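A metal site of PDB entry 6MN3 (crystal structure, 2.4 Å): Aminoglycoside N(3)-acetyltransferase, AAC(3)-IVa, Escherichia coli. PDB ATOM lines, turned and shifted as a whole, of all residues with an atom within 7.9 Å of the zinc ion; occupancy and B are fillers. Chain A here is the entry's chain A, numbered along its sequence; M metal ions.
The side-chain sulfur (SG) of Cys 191 sits close to the side-chain carboxylate (OE1) of Glu 193, 3.2 Å away. The side-chain sulfur (SG) of Cys 249 lies close to the backbone NH (N) of Glu 251, 3.5 Å away.
Within 4 Å of the zinc ion: Cys 191, His 243, Cys 249 and Cys 252. The nearest printed residue that does not touch the zinc ion is Glu 193 (4.5 Å).
ND1 of His 243 binds the zinc ion (2.2 Å). SG of Cys 191 binds the zinc ion, 2.3 Å away. SG of Cys 252 binds the zinc ion. SG of Cys 249 is bound to the zinc ion.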
ATOM      1  N   HIS A 190      21.987 -18.862  -1.815  1.00  0.00           N
ATOM      2  CA  HIS A 190      23.342 -19.311  -1.549  1.00  0.00           C
ATOM      3  C   HIS A 190      23.269 -20.603  -0.746  1.00  0.00           C
ATOM      4  O   HIS A 190      22.200 -21.213  -0.629  1.00  0.00           O
ATOM      5  CB  HIS A 190      24.158 -18.229  -0.829  1.00  0.00           C
ATOM      6  CG  HIS A 190      23.379 -17.495   0.226  1.00  0.00           C
ATOM      7  ND1 HIS A 190      23.393 -17.861   1.547  1.00  0.00           N
ATOM      8  CD2 HIS A 190      22.567 -16.403   0.144  1.00  0.00           C
ATOM      9  CE1 HIS A 190      22.618 -17.042   2.238  1.00  0.00           C
ATOM     10  NE2 HIS A 190      22.114 -16.151   1.404  1.00  0.00           N
ATOM     11  N   CYS A 191      24.400 -21.018  -0.194  1.00  0.00           N
ATOM     12  CA  CYS A 191      24.434 -22.253   0.595  1.00  0.00           C
ATOM     13  C   CYS A 191      23.642 -22.126   1.890  1.00  0.00           C
ATOM     14  O   CYS A 191      23.331 -23.155   2.509  1.00  0.00           O
ATOM     15  CB  CYS A 191      25.875 -22.636   0.911  1.00  0.00           C
ATOM     16  SG  CYS A 191      26.686 -21.560   2.103  1.00  0.00           S
ATOM     17  N   CYS A 192      23.322 -20.907   2.312  1.00  0.00           N
ATOM     18  CA  CYS A 192      22.530 -20.612   3.515  1.00  0.00           C
ATOM     19  C   CYS A 192      23.179 -21.113   4.797  1.00  0.00           C
ATOM     20  O   CYS A 192      22.569 -21.019   5.871  1.00  0.00           O
ATOM     21  CB  CYS A 192      21.112 -21.189   3.403  1.00  0.00           C
ATOM     22  SG  CYS A 192      20.149 -20.553   2.009  1.00  0.00           S
ATOM     23  N   GLU A 193      24.405 -21.627   4.725  1.00  0.00           N
ATOM     24  CA  GLU A 193      25.073 -22.124   5.928  1.00  0.00           C
ATOM     25  C   GLU A 193      25.354 -20.986   6.906  1.00  0.00           C
ATOM     26  O   GLU A 193      25.249 -21.170   8.118  1.00  0.00           O
ATOM     27  CB  GLU A 193      26.372 -22.837   5.544  1.00  0.00           C
ATOM     28  CG  GLU A 193      26.177 -24.249   5.045  1.00  0.00           C
ATOM     29  CD  GLU A 193      27.415 -24.799   4.369  1.00  0.00           C
ATOM     30  OE1 GLU A 193      27.649 -24.468   3.185  1.00  0.00           O
ATOM     31  OE2 GLU A 193      28.159 -25.563   5.013  1.00  0.00           O
ATOM     32  N   ARG A 194      25.711 -19.812   6.390  1.00  0.00           N
ATOM     33  CA  ARG A 194      26.019 -18.661   7.247  1.00  0.00           C
ATOM     34  C   ARG A 194      24.793 -18.092   7.925  1.00  0.00           C
ATOM     35  O   ARG A 194      24.934 -17.158   8.721  1.00  0.00           O
ATOM     36  CB  ARG A 194      26.716 -17.581   6.429  1.00  0.00           C
ATOM     37  CG  ARG A 194      28.030 -18.029   5.793  1.00  0.00           C
ATOM     38  CD  ARG A 194      29.216 -17.519   6.583  1.00  0.00           C
ATOM     39  NE  ARG A 194      29.355 -16.063   6.497  1.00  0.00           N
ATOM     40  CZ  ARG A 194      30.349 -15.379   7.044  1.00  0.00           C
ATOM     41  NH1 ARG A 194      31.296 -15.998   7.718  1.00  0.00           N
ATOM     42  NH2 ARG A 194      30.389 -14.052   6.916  1.00  0.00           N
ATOM     43  N   PHE A 241      26.085 -12.826   5.137  1.00  0.00           N
ATOM     44  CA  PHE A 241      25.652 -14.196   4.951  1.00  0.00           C
ATOM     45  C   PHE A 241      26.434 -14.936   3.873  1.00  0.00           C
ATOM     46  O   PHE A 241      26.131 -16.098   3.592  1.00  0.00           O
ATOM     47  CB  PHE A 241      24.156 -14.223   4.598  1.00  0.00           C
ATOM     48  CG  PHE A 241      23.261 -13.798   5.726  1.00  0.00           C
ATOM     49  CD1 PHE A 241      23.542 -14.166   7.028  1.00  0.00           C
ATOM     50  CD2 PHE A 241      22.121 -13.046   5.476  1.00  0.00           C
ATOM     51  CE1 PHE A 241      22.714 -13.775   8.074  1.00  0.00           C
ATOM     52  CE2 PHE A 241      21.288 -12.663   6.510  1.00  0.00           C
ATOM     53  CZ  PHE A 241      21.590 -13.023   7.809  1.00  0.00           C
ATOM     54  N   LEU A 242      27.418 -14.286   3.252  1.00  0.00           N
ATOM     55  CA  LEU A 242      28.193 -14.888   2.171  1.00  0.00           C
ATOM     56  C   LEU A 242      29.483 -15.488   2.725  1.00  0.00           C
ATOM     57  O   LEU A 242      30.227 -14.813   3.456  1.00  0.00           O
ATOM     58  CB  LEU A 242      28.520 -13.856   1.086  1.00  0.00           C
ATOM     59  CG  LEU A 242      27.369 -13.344   0.223  1.00  0.00           C
ATOM     60  CD1 LEU A 242      27.921 -12.687  -1.030  1.00  0.00           C
ATOM     61  CD2 LEU A 242      26.409 -14.468  -0.125  1.00  0.00           C
ATOM     62  N   HIS A 243      29.746 -16.732   2.364  1.00  0.00           N
ATOM     63  CA  HIS A 243      31.023 -17.341   2.703  1.00  0.00           C
ATOM     64  C   HIS A 243      32.153 -16.546   2.062  1.00  0.00           C
ATOM     65  O   HIS A 243      32.028 -16.116   0.908  1.00  0.00           O
ATOM     66  CB  HIS A 243      31.080 -18.791   2.221  1.00  0.00           C
ATOM     67  CG  HIS A 243      30.682 -19.792   3.270  1.00  0.00           C
ATOM     68  ND1 HIS A 243      29.464 -20.438   3.257  1.00  0.00           N
ATOM     69  CD2 HIS A 243      31.353 -20.268   4.339  1.00  0.00           C
ATOM     70  CE1 HIS A 243      29.394 -21.263   4.288  1.00  0.00           C
ATOM     71  NE2 HIS A 243      30.529 -21.185   4.957  1.00  0.00           N
ATOM     72  N   PRO A 244      33.261 -16.326   2.769  1.00  0.00           N
ATOM     73  CA  PRO A 244      34.385 -15.650   2.150  1.00  0.00           C
ATOM     74  C   PRO A 244      34.968 -16.515   1.047  1.00  0.00           C
ATOM     75  O   PRO A 244      34.807 -17.749   1.052  1.00  0.00           O
ATOM     76  CB  PRO A 244      35.373 -15.461   3.300  1.00  0.00           C
ATOM     77  CG  PRO A 244      34.998 -16.496   4.301  1.00  0.00           C
ATOM     78  CD  PRO A 244      33.508 -16.641   4.182  1.00  0.00           C
ATOM     79  N   ALA A 247      36.868 -19.787   2.125  1.00  0.00           N
ATOM     80  CA  ALA A 247      36.138 -21.031   2.336  1.00  0.00           C
ATOM     81  C   ALA A 247      35.833 -21.741   1.024  1.00  0.00           C
ATOM     82  O   ALA A 247      35.554 -22.948   1.047  1.00  0.00           O
ATOM     83  CB  ALA A 247      34.844 -20.752   3.100  1.00  0.00           C
ATOM     84  N   GLY A 248      35.874 -21.035  -0.098  1.00  0.00           N
ATOM     85  CA  GLY A 248      35.699 -21.669  -1.391  1.00  0.00           C
ATOM     86  C   GLY A 248      34.330 -22.271  -1.609  1.00  0.00           C
ATOM     87  O   GLY A 248      34.220 -23.348  -2.218  1.00  0.00           O
ATOM     88  N   CYS A 249      33.285 -21.615  -1.127  1.00  0.00           N
ATOM     89  CA  CYS A 249      31.928 -22.113  -1.308  1.00  0.00           C
ATOM     90  C   CYS A 249      31.472 -21.840  -2.739  1.00  0.00           C
ATOM     91  O   CYS A 249      31.488 -20.694  -3.192  1.00  0.00           O
ATOM     92  CB  CYS A 249      30.976 -21.471  -0.307  1.00  0.00           C
ATOM     93  SG  CYS A 249      29.263 -21.996  -0.506  1.00  0.00           S
ATOM     94  N   GLU A 250      31.063 -22.894  -3.444  1.00  0.00           N
ATOM     95  CA  GLU A 250      30.583 -22.738  -4.806  1.00  0.00           C
ATOM     96  C   GLU A 250      29.249 -22.021  -4.851  1.00  0.00           C
ATOM     97  O   GLU A 250      28.998 -21.235  -5.784  1.00  0.00           O
ATOM     98  CB  GLU A 250      30.475 -24.114  -5.479  1.00  0.00           C
ATOM     99  CG  GLU A 250      30.714 -24.092  -6.988  1.00  0.00           C
ATOM    100  CD  GLU A 250      31.089 -25.449  -7.530  1.00  0.00           C
ATOM    101  OE1 GLU A 250      30.866 -25.699  -8.733  1.00  0.00           O
ATOM    102  OE2 GLU A 250      31.615 -26.279  -6.749  1.00  0.00           O
ATOM    103  N   GLU A 251      28.378 -22.256  -3.864  1.00  0.00           N
ATOM    104  CA  GLU A 251      27.070 -21.617  -3.864  1.00  0.00           C
ATOM    105  C   GLU A 251      27.142 -20.154  -3.446  1.00  0.00           C
ATOM    106  O   GLU A 251      26.297 -19.356  -3.849  1.00  0.00           O
ATOM    107  CB  GLU A 251      26.123 -22.385  -2.943  1.00  0.00           C
ATOM    108  CG  GLU A 251      24.702 -22.511  -3.463  1.00  0.00           C
ATOM    109  CD  GLU A 251      23.978 -23.715  -2.899  1.00  0.00           C
ATOM    110  OE1 GLU A 251      22.758 -23.603  -2.632  1.00  0.00           O
ATOM    111  OE2 GLU A 251      24.615 -24.767  -2.716  1.00  0.00           O
ATOM    112  N   CYS A 252      28.148 -19.781  -2.646  1.00  0.00           N
ATOM    113  CA  CYS A 252      28.287 -18.403  -2.185  1.00  0.00           C
ATOM    114  C   CYS A 252      29.082 -17.543  -3.156  1.00  0.00           C
ATOM    115  O   CYS A 252      28.713 -16.389  -3.394  1.00  0.00           O
ATOM    116  CB  CYS A 252      28.938 -18.374  -0.806  1.00  0.00           C
ATOM    117  SG  CYS A 252      27.771 -18.439   0.567  1.00  0.00           S
ATOM    118  N   ASP A 253      30.167 -18.082  -3.723  1.00  0.00           N
ATOM    119  CA  ASP A 253      30.945 -17.315  -4.684  1.00  0.00           C
ATOM    120  C   ASP A 253      30.139 -16.980  -5.938  1.00  0.00           C
ATOM    121  O   ASP A 253      30.458 -16.001  -6.617  1.00  0.00           O
ATOM    122  CB  ASP A 253      32.207 -18.086  -5.064  1.00  0.00           C
ATOM    123  CG  ASP A 253      33.234 -18.125  -3.947  1.00  0.00           C
ATOM    124  OD1 ASP A 253      33.026 -17.419  -2.937  1.00  0.00           O
ATOM    125  OD2 ASP A 253      34.240 -18.846  -4.081  1.00  0.00           O
HETATM  126 ZN    ZN M   1      28.606 -20.531   1.250  1.00  0.00          ZN
